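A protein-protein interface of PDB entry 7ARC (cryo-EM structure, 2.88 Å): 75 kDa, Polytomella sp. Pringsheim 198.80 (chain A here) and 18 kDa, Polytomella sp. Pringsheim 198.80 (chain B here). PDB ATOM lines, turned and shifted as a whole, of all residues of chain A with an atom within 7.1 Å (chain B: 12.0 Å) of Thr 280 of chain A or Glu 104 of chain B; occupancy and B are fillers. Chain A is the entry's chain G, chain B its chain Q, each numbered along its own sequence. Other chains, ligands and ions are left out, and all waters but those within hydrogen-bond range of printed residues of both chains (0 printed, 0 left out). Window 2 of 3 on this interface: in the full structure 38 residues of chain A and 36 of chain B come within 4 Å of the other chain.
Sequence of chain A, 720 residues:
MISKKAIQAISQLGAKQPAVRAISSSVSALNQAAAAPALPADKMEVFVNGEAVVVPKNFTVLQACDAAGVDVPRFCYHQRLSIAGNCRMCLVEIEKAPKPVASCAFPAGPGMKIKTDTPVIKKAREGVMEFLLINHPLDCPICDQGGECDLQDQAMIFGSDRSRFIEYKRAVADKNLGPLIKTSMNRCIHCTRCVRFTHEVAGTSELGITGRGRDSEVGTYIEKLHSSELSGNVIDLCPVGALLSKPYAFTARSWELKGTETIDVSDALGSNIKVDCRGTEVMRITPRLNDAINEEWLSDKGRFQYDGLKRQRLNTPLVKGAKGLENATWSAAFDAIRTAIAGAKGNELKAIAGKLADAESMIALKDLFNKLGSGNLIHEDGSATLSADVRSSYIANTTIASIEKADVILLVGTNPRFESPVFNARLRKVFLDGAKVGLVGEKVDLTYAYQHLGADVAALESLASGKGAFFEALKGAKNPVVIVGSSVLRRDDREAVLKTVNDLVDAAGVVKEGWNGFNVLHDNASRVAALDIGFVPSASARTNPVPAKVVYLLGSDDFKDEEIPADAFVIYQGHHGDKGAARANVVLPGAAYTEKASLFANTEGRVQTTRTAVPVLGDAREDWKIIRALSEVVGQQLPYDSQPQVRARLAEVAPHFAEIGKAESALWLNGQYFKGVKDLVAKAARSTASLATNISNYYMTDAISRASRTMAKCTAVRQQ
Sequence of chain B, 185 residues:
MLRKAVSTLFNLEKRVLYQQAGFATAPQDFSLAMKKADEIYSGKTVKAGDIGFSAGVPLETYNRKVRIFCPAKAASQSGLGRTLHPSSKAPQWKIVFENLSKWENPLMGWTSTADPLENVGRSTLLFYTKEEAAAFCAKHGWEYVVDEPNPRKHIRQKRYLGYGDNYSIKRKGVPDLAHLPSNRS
The side-chain hydroxyl of Thr 280 of chain A sits at hydrogen-bond distance from the side-chain carboxylate of Glu 104 of chain B, 3.1 Å away.
The side-chain amide nitrogen of Asn 99 of chain B lies within hydrogen-bond range of the backbone carbonyl oxygen of Ala 613 of chain A (3.2 Å).
NZ of Lys 102 of chain B is in salt-bridge range of OE2 of Glu 118 of chain B, 3.9 Å away.
Gly 279 of chain A touches Thr 111 of chain B.
Thr 280 of chain A touches Lys 102 of chain B.
CB of Pro 615 of chain A touches O of Leu 100 of chain B, 3.7 Å away.
CG of Pro 615 of chain A touches N of Lys 102 of chain B, 3.8 Å away.
Cys 277 of chain A touches none of the printed residues of chain B.
Arg 278 of chain A touches none of the printed residues of chain B.
Of chain B, only Thr 111 (3.9 Å) comes within 4 Å of Gly 279 of chain A.
Of chain B, only Lys 102 and Glu 104 come within 4 Å of Thr 280 of chain A.
No residue of chain B comes within 4 Å of Val 282 of chain A.
No residue of chain B comes within 4 Å of Val 614 of chain A.
Of chain B, only Leu 100 (3.7 Å) and Lys 102 (3.8 Å) come within 4 Å of Pro 615 of chain A.
Printed residues of chain A within 4 Å of Leu 100 of chain B: Pro 615 (3.7 Å).
Of the printed residues of chain A, Lys 102 of chain B touches Thr 280 (3.6 Å) and Pro 615 (3.8 Å).
Pro 106 of chain B touches none of the printed residues of chain A.
The nearest printed residue of chain B that does not touch Thr 280 of chain A is Trp 103 of chain B (4.5 Å).
The nearest residue of chain A that does not touch Glu 104 of chain B is Gly 279 of chain A (5.7 Å).
Of the 19 printed residues of chain B, 5 touch a printed residue of chain A.
Of the 12 printed residues of chain A, 4 touch a printed residue of chain B.
Hydrophobic or aromatic side chains of chain A within 4 Å of the printed part of chain B: Pro 615.
Among the printed residues, no Asp or Glu carboxylate lies within 4 Å of a Lys or Arg side-chain nitrogen of the other chain.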
ATOM      1  N   CYS A 277       2.299  22.904  -7.201  1.00  0.00           N
ATOM      2  CA  CYS A 277       0.973  22.735  -6.630  1.00  0.00           C
ATOM      3  C   CYS A 277      -0.040  23.556  -7.406  1.00  0.00           C
ATOM      4  O   CYS A 277       0.242  24.685  -7.814  1.00  0.00           O
ATOM      5  CB  CYS A 277       0.949  23.162  -5.163  1.00  0.00           C
ATOM      6  SG  CYS A 277       2.314  22.524  -4.191  1.00  0.00           S
ATOM      7  N   ARG A 278      -1.219  22.980  -7.611  1.00  0.00           N
ATOM      8  CA  ARG A 278      -2.386  23.709  -8.082  1.00  0.00           C
ATOM      9  C   ARG A 278      -3.427  23.713  -6.971  1.00  0.00           C
ATOM     10  O   ARG A 278      -3.952  22.656  -6.608  1.00  0.00           O
ATOM     11  CB  ARG A 278      -2.937  23.086  -9.362  1.00  0.00           C
ATOM     12  CG  ARG A 278      -4.084  23.845  -9.984  1.00  0.00           C
ATOM     13  CD  ARG A 278      -4.541  23.157 -11.250  1.00  0.00           C
ATOM     14  NE  ARG A 278      -5.139  21.857 -10.983  1.00  0.00           N
ATOM     15  CZ  ARG A 278      -5.463  20.982 -11.923  1.00  0.00           C
ATOM     16  NH1 ARG A 278      -5.273  21.243 -13.204  1.00  0.00           N
ATOM     17  NH2 ARG A 278      -5.992  19.815 -11.567  1.00  0.00           N
ATOM     18  N   GLY A 279      -3.732  24.896  -6.451  1.00  0.00           N
ATOM     19  CA  GLY A 279      -4.655  24.985  -5.331  1.00  0.00           C
ATOM     20  C   GLY A 279      -4.104  24.280  -4.107  1.00  0.00           C
ATOM     21  O   GLY A 279      -2.991  24.559  -3.649  1.00  0.00           O
ATOM     22  N   THR A 280      -4.888  23.353  -3.565  1.00  0.00           N
ATOM     23  CA  THR A 280      -4.511  22.595  -2.381  1.00  0.00           C
ATOM     24  C   THR A 280      -3.895  21.243  -2.715  1.00  0.00           C
ATOM     25  O   THR A 280      -3.658  20.441  -1.807  1.00  0.00           O
ATOM     26  CB  THR A 280      -5.725  22.388  -1.474  1.00  0.00           C
ATOM     27  OG1 THR A 280      -6.722  21.639  -2.179  1.00  0.00           O
ATOM     28  CG2 THR A 280      -6.310  23.720  -1.057  1.00  0.00           C
ATOM     29  N   GLU A 281      -3.628  20.973  -3.987  1.00  0.00           N
ATOM     30  CA  GLU A 281      -3.138  19.677  -4.436  1.00  0.00           C
ATOM     31  C   GLU A 281      -1.703  19.794  -4.927  1.00  0.00           C
ATOM     32  O   GLU A 281      -1.385  20.688  -5.716  1.00  0.00           O
ATOM     33  CB  GLU A 281      -4.025  19.127  -5.554  1.00  0.00           C
ATOM     34  CG  GLU A 281      -3.631  17.746  -6.031  1.00  0.00           C
ATOM     35  CD  GLU A 281      -4.553  17.216  -7.107  1.00  0.00           C
ATOM     36  OE1 GLU A 281      -5.494  17.941  -7.495  1.00  0.00           O
ATOM     37  OE2 GLU A 281      -4.331  16.081  -7.576  1.00  0.00           O
ATOM     38  N   VAL A 282      -0.844  18.894  -4.458  1.00  0.00           N
ATOM     39  CA  VAL A 282       0.491  18.737  -5.024  1.00  0.00           C
ATOM     40  C   VAL A 282       0.357  17.962  -6.328  1.00  0.00           C
ATOM     41  O   VAL A 282      -0.207  16.863  -6.351  1.00  0.00           O
ATOM     42  CB  VAL A 282       1.428  18.016  -4.045  1.00  0.00           C
ATOM     43  CG1 VAL A 282       2.738  17.670  -4.721  1.00  0.00           C
ATOM     44  CG2 VAL A 282       1.668  18.869  -2.815  1.00  0.00           C
ATOM     45  N   LYS A 310      -2.386  11.912  -0.707  1.00  0.00           N
ATOM     46  CA  LYS A 310      -3.811  12.157  -0.840  1.00  0.00           C
ATOM     47  C   LYS A 310      -4.644  11.044  -0.228  1.00  0.00           C
ATOM     48  O   LYS A 310      -5.875  11.110  -0.279  1.00  0.00           O
ATOM     49  CB  LYS A 310      -4.189  12.295  -2.320  1.00  0.00           C
ATOM     50  CG  LYS A 310      -3.896  13.640  -2.959  1.00  0.00           C
ATOM     51  CD  LYS A 310      -2.406  13.811  -3.186  1.00  0.00           C
ATOM     52  CE  LYS A 310      -2.081  15.097  -3.907  1.00  0.00           C
ATOM     53  NZ  LYS A 310      -0.609  15.281  -4.007  1.00  0.00           N
ATOM     54  N   GLU A 595       3.536  20.425   3.998  1.00  0.00           N
ATOM     55  CA  GLU A 595       2.612  21.357   4.622  1.00  0.00           C
ATOM     56  C   GLU A 595       3.214  22.131   5.785  1.00  0.00           C
ATOM     57  O   GLU A 595       2.493  22.894   6.436  1.00  0.00           O
ATOM     58  CB  GLU A 595       1.375  20.592   5.102  1.00  0.00           C
ATOM     59  CG  GLU A 595       0.541  20.025   3.977  1.00  0.00           C
ATOM     60  CD  GLU A 595      -0.665  19.256   4.469  1.00  0.00           C
ATOM     61  OE1 GLU A 595      -0.783  19.056   5.695  1.00  0.00           O
ATOM     62  OE2 GLU A 595      -1.496  18.852   3.628  1.00  0.00           O
ATOM     63  N   ALA A 613       4.286  24.096   1.025  1.00  0.00           N
ATOM     64  CA  ALA A 613       3.810  24.118  -0.352  1.00  0.00           C
ATOM     65  C   ALA A 613       2.291  24.209  -0.408  1.00  0.00           C
ATOM     66  O   ALA A 613       1.739  24.997  -1.185  1.00  0.00           O
ATOM     67  CB  ALA A 613       4.302  22.880  -1.098  1.00  0.00           C
ATOM     68  N   VAL A 614       1.598  23.419   0.407  1.00  0.00           N
ATOM     69  CA  VAL A 614       0.139  23.399   0.420  1.00  0.00           C
ATOM     70  C   VAL A 614      -0.339  23.572   1.856  1.00  0.00           C
ATOM     71  O   VAL A 614       0.384  23.214   2.796  1.00  0.00           O
ATOM     72  CB  VAL A 614      -0.415  22.107  -0.206  1.00  0.00           C
ATOM     73  CG1 VAL A 614      -0.009  22.000  -1.656  1.00  0.00           C
ATOM     74  CG2 VAL A 614       0.072  20.899   0.559  1.00  0.00           C
ATOM     75  N   PRO A 615      -1.532  24.116   2.078  1.00  0.00           N
ATOM     76  CA  PRO A 615      -2.005  24.333   3.448  1.00  0.00           C
ATOM     77  C   PRO A 615      -2.353  23.028   4.147  1.00  0.00           C
ATOM     78  O   PRO A 615      -2.576  21.988   3.525  1.00  0.00           O
ATOM     79  CB  PRO A 615      -3.241  25.214   3.259  1.00  0.00           C
ATOM     80  CG  PRO A 615      -3.738  24.858   1.911  1.00  0.00           C
ATOM     81  CD  PRO A 615      -2.513  24.586   1.082  1.00  0.00           C
ATOM     82  N   LEU A 617      -4.392  20.225   6.169  1.00  0.00           N
ATOM     83  CA  LEU A 617      -5.683  19.635   5.852  1.00  0.00           C
ATOM     84  C   LEU A 617      -6.525  19.465   7.106  1.00  0.00           C
ATOM     85  O   LEU A 617      -6.041  18.956   8.122  1.00  0.00           O
ATOM     86  CB  LEU A 617      -5.492  18.274   5.186  1.00  0.00           C
ATOM     87  CG  LEU A 617      -6.772  17.574   4.744  1.00  0.00           C
ATOM     88  CD1 LEU A 617      -7.503  18.380   3.683  1.00  0.00           C
ATOM     89  CD2 LEU A 617      -6.460  16.179   4.266  1.00  0.00           C
ATOM     90  N   ASN B  99       2.475  30.880   2.632  1.00  0.00           N
ATOM     91  CA  ASN B  99       1.201  30.369   2.148  1.00  0.00           C
ATOM     92  C   ASN B  99       0.217  30.220   3.299  1.00  0.00           C
ATOM     93  O   ASN B  99       0.584  29.802   4.400  1.00  0.00           O
ATOM     94  CB  ASN B  99       1.402  29.023   1.454  1.00  0.00           C
ATOM     95  CG  ASN B  99       2.040  29.166   0.088  1.00  0.00           C
ATOM     96  OD1 ASN B  99       2.156  30.270  -0.442  1.00  0.00           O
ATOM     97  ND2 ASN B  99       2.464  28.048  -0.486  1.00  0.00           N
ATOM     98  N   LEU B 100      -1.039  30.564   3.038  1.00  0.00           N
ATOM     99  CA  LEU B 100      -2.085  30.528   4.049  1.00  0.00           C
ATOM    100  C   LEU B 100      -3.181  29.548   3.631  1.00  0.00           C
ATOM    101  O   LEU B 100      -3.057  28.829   2.637  1.00  0.00           O
ATOM    102  CB  LEU B 100      -2.636  31.936   4.278  1.00  0.00           C
ATOM    103  CG  LEU B 100      -1.713  32.892   5.035  1.00  0.00           C
ATOM    104  CD1 LEU B 100      -2.440  34.178   5.372  1.00  0.00           C
ATOM    105  CD2 LEU B 100      -1.159  32.240   6.289  1.00  0.00           C
ATOM    106  N   SER B 101      -4.263  29.527   4.405  1.00  0.00           N
ATOM    107  CA  SER B 101      -5.315  28.537   4.212  1.00  0.00           C
ATOM    108  C   SER B 101      -6.022  28.699   2.870  1.00  0.00           C
ATOM    109  O   SER B 101      -6.234  29.811   2.383  1.00  0.00           O
ATOM    110  CB  SER B 101      -6.335  28.625   5.345  1.00  0.00           C
ATOM    111  OG  SER B 101      -7.037  29.853   5.305  1.00  0.00           O
ATOM    112  N   LYS B 102      -6.386  27.563   2.281  1.00  0.00           N
ATOM    113  CA  LYS B 102      -7.145  27.486   1.044  1.00  0.00           C
ATOM    114  C   LYS B 102      -8.166  26.371   1.191  1.00  0.00           C
ATOM    115  O   LYS B 102      -7.862  25.323   1.763  1.00  0.00           O
ATOM    116  CB  LYS B 102      -6.253  27.202  -0.166  1.00  0.00           C
ATOM    117  CG  LYS B 102      -5.268  28.290  -0.507  1.00  0.00           C
ATOM    118  CD  LYS B 102      -4.456  27.900  -1.723  1.00  0.00           C
ATOM    119  CE  LYS B 102      -3.517  29.011  -2.131  1.00  0.00           C
ATOM    120  NZ  LYS B 102      -2.460  29.236  -1.110  1.00  0.00           N
ATOM    121  N   TRP B 103      -9.374  26.593   0.684  1.00  0.00           N
ATOM    122  CA  TRP B 103     -10.418  25.585   0.770  1.00  0.00           C
ATOM    123  C   TRP B 103     -11.138  25.511  -0.565  1.00  0.00           C
ATOM    124  O   TRP B 103     -10.802  26.218  -1.519  1.00  0.00           O
ATOM    125  CB  TRP B 103     -11.393  25.863   1.922  1.00  0.00           C
ATOM    126  CG  TRP B 103     -12.131  27.154   1.858  1.00  0.00           C
ATOM    127  CD1 TRP B 103     -13.416  27.339   1.455  1.00  0.00           C
ATOM    128  CD2 TRP B 103     -11.643  28.442   2.243  1.00  0.00           C
ATOM    129  NE1 TRP B 103     -13.756  28.661   1.549  1.00  0.00           N
ATOM    130  CE2 TRP B 103     -12.683  29.361   2.031  1.00  0.00           C
ATOM    131  CE3 TRP B 103     -10.423  28.908   2.738  1.00  0.00           C
ATOM    132  CZ2 TRP B 103     -12.544  30.717   2.294  1.00  0.00           C
ATOM    133  CZ3 TRP B 103     -10.288  30.251   2.999  1.00  0.00           C
ATOM    134  CH2 TRP B 103     -11.340  31.140   2.776  1.00  0.00           C
ATOM    135  N   GLU B 104     -12.133  24.636  -0.631  1.00  0.00           N
ATOM    136  CA  GLU B 104     -12.867  24.360  -1.856  1.00  0.00           C
ATOM    137  C   GLU B 104     -14.271  24.922  -1.729  1.00  0.00           C
ATOM    138  O   GLU B 104     -14.934  24.722  -0.706  1.00  0.00           O
ATOM    139  CB  GLU B 104     -12.921  22.858  -2.140  1.00  0.00           C
ATOM    140  CG  GLU B 104     -11.573  22.172  -2.060  1.00  0.00           C
ATOM    141  CD  GLU B 104     -10.713  22.438  -3.275  1.00  0.00           C
ATOM    142  OE1 GLU B 104      -9.504  22.702  -3.102  1.00  0.00           O
ATOM    143  OE2 GLU B 104     -11.241  22.380  -4.405  1.00  0.00           O
ATOM    144  N   ASN B 105     -14.712  25.628  -2.758  1.00  0.00           N
ATOM    145  CA  ASN B 105     -16.068  26.148  -2.777  1.00  0.00           C
ATOM    146  C   ASN B 105     -17.058  24.993  -2.676  1.00  0.00           C
ATOM    147  O   ASN B 105     -16.989  24.054  -3.477  1.00  0.00           O
ATOM    148  CB  ASN B 105     -16.305  26.945  -4.057  1.00  0.00           C
ATOM    149  CG  ASN B 105     -17.608  27.702  -4.036  1.00  0.00           C
ATOM    150  OD1 ASN B 105     -18.035  28.194  -2.995  1.00  0.00           O
ATOM    151  ND2 ASN B 105     -18.246  27.810  -5.192  1.00  0.00           N
ATOM    152  N   PRO B 106     -17.974  25.014  -1.706  1.00  0.00           N
ATOM    153  CA  PRO B 106     -18.925  23.901  -1.575  1.00  0.00           C
ATOM    154  C   PRO B 106     -19.782  23.675  -2.808  1.00  0.00           C
ATOM    155  O   PRO B 106     -20.138  22.526  -3.092  1.00  0.00           O
ATOM    156  CB  PRO B 106     -19.771  24.303  -0.357  1.00  0.00           C
ATOM    157  CG  PRO B 106     -19.556  25.764  -0.191  1.00  0.00           C
ATOM    158  CD  PRO B 106     -18.170  26.036  -0.666  1.00  0.00           C
ATOM    159  N   LEU B 107     -20.123  24.727  -3.551  1.00  0.00           N
ATOM    160  CA  LEU B 107     -21.009  24.564  -4.698  1.00  0.00           C
ATOM    161  C   LEU B 107     -20.268  24.060  -5.932  1.00  0.00           C
ATOM    162  O   LEU B 107     -20.722  23.121  -6.594  1.00  0.00           O
ATOM    163  CB  LEU B 107     -21.708  25.886  -5.007  1.00  0.00           C
ATOM    164  CG  LEU B 107     -22.860  25.820  -6.009  1.00  0.00           C
ATOM    165  CD1 LEU B 107     -24.110  25.268  -5.358  1.00  0.00           C
ATOM    166  CD2 LEU B 107     -23.122  27.189  -6.593  1.00  0.00           C
ATOM    167  N   MET B 108     -19.129  24.663  -6.261  1.00  0.00           N
ATOM    168  CA  MET B 108     -18.451  24.376  -7.515  1.00  0.00           C
ATOM    169  C   MET B 108     -17.032  23.857  -7.346  1.00  0.00           C
ATOM    170  O   MET B 108     -16.347  23.647  -8.352  1.00  0.00           O
ATOM    171  CB  MET B 108     -18.423  25.629  -8.401  1.00  0.00           C
ATOM    172  CG  MET B 108     -19.736  25.931  -9.100  1.00  0.00           C
ATOM    173  SD  MET B 108     -20.050  24.853 -10.508  1.00  0.00           S
ATOM    174  CE  MET B 108     -19.329  25.810 -11.832  1.00  0.00           C
ATOM    175  N   GLY B 109     -16.578  23.618  -6.118  1.00  0.00           N
ATOM    176  CA  GLY B 109     -15.258  23.056  -5.916  1.00  0.00           C
ATOM    177  C   GLY B 109     -14.114  23.961  -6.301  1.00  0.00           C
ATOM    178  O   GLY B 109     -12.982  23.489  -6.423  1.00  0.00           O
ATOM    179  N   TRP B 110     -14.377  25.246  -6.501  1.00  0.00           N
ATOM    180  CA  TRP B 110     -13.328  26.208  -6.788  1.00  0.00           C
ATOM    181  C   TRP B 110     -12.454  26.429  -5.560  1.00  0.00           C
ATOM    182  O   TRP B 110     -12.894  26.266  -4.421  1.00  0.00           O
ATOM    183  CB  TRP B 110     -13.946  27.530  -7.228  1.00  0.00           C
ATOM    184  CG  TRP B 110     -14.600  27.444  -8.554  1.00  0.00           C
ATOM    185  CD1 TRP B 110     -14.346  26.535  -9.533  1.00  0.00           C
ATOM    186  CD2 TRP B 110     -15.651  28.278  -9.043  1.00  0.00           C
ATOM    187  NE1 TRP B 110     -15.162  26.761 -10.610  1.00  0.00           N
ATOM    188  CE2 TRP B 110     -15.975  27.827 -10.333  1.00  0.00           C
ATOM    189  CE3 TRP B 110     -16.346  29.369  -8.515  1.00  0.00           C
ATOM    190  CZ2 TRP B 110     -16.959  28.428 -11.107  1.00  0.00           C
ATOM    191  CZ3 TRP B 110     -17.322  29.963  -9.283  1.00  0.00           C
ATOM    192  CH2 TRP B 110     -17.621  29.494 -10.564  1.00  0.00           C
ATOM    193  N   THR B 111     -11.200  26.798  -5.801  1.00  0.00           N
ATOM    194  CA  THR B 111     -10.261  27.061  -4.717  1.00  0.00           C
ATOM    195  C   THR B 111     -10.521  28.452  -4.151  1.00  0.00           C
ATOM    196  O   THR B 111     -10.333  29.457  -4.841  1.00  0.00           O
ATOM    197  CB  THR B 111      -8.823  26.932  -5.205  1.00  0.00           C
ATOM    198  OG1 THR B 111      -8.701  25.762  -6.022  1.00  0.00           O
ATOM    199  CG2 THR B 111      -7.877  26.817  -4.026  1.00  0.00           C
ATOM    200  N   SER B 112     -10.950  28.512  -2.897  1.00  0.00           N
ATOM    201  CA  SER B 112     -11.267  29.764  -2.230  1.00  0.00           C
ATOM    202  C   SER B 112     -10.135  30.151  -1.288  1.00  0.00           C
ATOM    203  O   SER B 112      -9.426  29.294  -0.758  1.00  0.00           O
ATOM    204  CB  SER B 112     -12.576  29.648  -1.451  1.00  0.00           C
ATOM    205  OG  SER B 112     -13.666  29.415  -2.321  1.00  0.00           O
ATOM    206  N   THR B 113      -9.965  31.456  -1.087  1.00  0.00           N
ATOM    207  CA  THR B 113      -8.878  31.948  -0.257  1.00  0.00           C
ATOM    208  C   THR B 113      -9.317  33.224   0.443  1.00  0.00           C
ATOM    209  O   THR B 113     -10.271  33.887   0.030  1.00  0.00           O
ATOM    210  CB  THR B 113      -7.609  32.210  -1.074  1.00  0.00           C
ATOM    211  OG1 THR B 113      -6.527  32.520  -0.190  1.00  0.00           O
ATOM    212  CG2 THR B 113      -7.821  33.381  -2.013  1.00  0.00           C
ATOM    213  N   ALA B 114      -8.615  33.552   1.526  1.00  0.00           N
ATOM    214  CA  ALA B 114      -8.791  34.823   2.214  1.00  0.00           C
ATOM    215  C   ALA B 114      -7.495  35.614   2.319  1.00  0.00           C
ATOM    216  O   ALA B 114      -7.432  36.581   3.085  1.00  0.00           O
ATOM    217  CB  ALA B 114      -9.373  34.599   3.609  1.00  0.00           C
ATOM    218  N   ASP B 115      -6.458  35.224   1.580  1.00  0.00           N
ATOM    219  CA  ASP B 115      -5.161  35.877   1.668  1.00  0.00           C
ATOM    220  C   ASP B 115      -5.102  37.013   0.656  1.00  0.00           C
ATOM    221  O   ASP B 115      -5.123  36.748  -0.555  1.00  0.00           O
ATOM    222  CB  ASP B 115      -4.045  34.877   1.409  1.00  0.00           C
ATOM    223  CG  ASP B 115      -2.678  35.421   1.765  1.00  0.00           C
ATOM    224  OD1 ASP B 115      -2.606  36.505   2.380  1.00  0.00           O
ATOM    225  OD2 ASP B 115      -1.673  34.761   1.429  1.00  0.00           O
ATOM    226  N   GLU B 118      -1.767  36.940  -1.785  1.00  0.00           N
ATOM    227  CA  GLU B 118      -1.468  35.612  -2.308  1.00  0.00           C
ATOM    228  C   GLU B 118      -0.532  35.678  -3.509  1.00  0.00           C
ATOM    229  O   GLU B 118       0.483  34.973  -3.557  1.00  0.00           O
ATOM    230  CB  GLU B 118      -2.757  34.891  -2.687  1.00  0.00           C
ATOM    231  CG  GLU B 118      -2.507  33.484  -3.170  1.00  0.00           C
ATOM    232  CD  GLU B 118      -3.774  32.746  -3.508  1.00  0.00           C
ATOM    233  OE1 GLU B 118      -4.862  33.340  -3.381  1.00  0.00           O
ATOM    234  OE2 GLU B 118      -3.674  31.577  -3.927  1.00  0.00           O
ATOM    235  N   ARG B 122       4.705  37.117  -5.980  1.00  0.00           N
ATOM    236  CA  ARG B 122       5.167  36.285  -7.086  1.00  0.00           C
ATOM    237  C   ARG B 122       5.038  37.017  -8.417  1.00  0.00           C
ATOM    238  O   ARG B 122       5.921  36.918  -9.277  1.00  0.00           O
ATOM    239  CB  ARG B 122       4.389  34.968  -7.101  1.00  0.00           C
ATOM    240  CG  ARG B 122       2.905  35.162  -7.345  1.00  0.00           C
ATOM    241  CD  ARG B 122       2.078  33.890  -7.357  1.00  0.00           C
ATOM    242  NE  ARG B 122       2.399  33.041  -8.495  1.00  0.00           N
ATOM    243  CZ  ARG B 122       2.026  31.774  -8.608  1.00  0.00           C
ATOM    244  NH1 ARG B 122       1.249  31.202  -7.705  1.00  0.00           N
ATOM    245  NH2 ARG B 122       2.420  31.074  -9.666  1.00  0.00           N
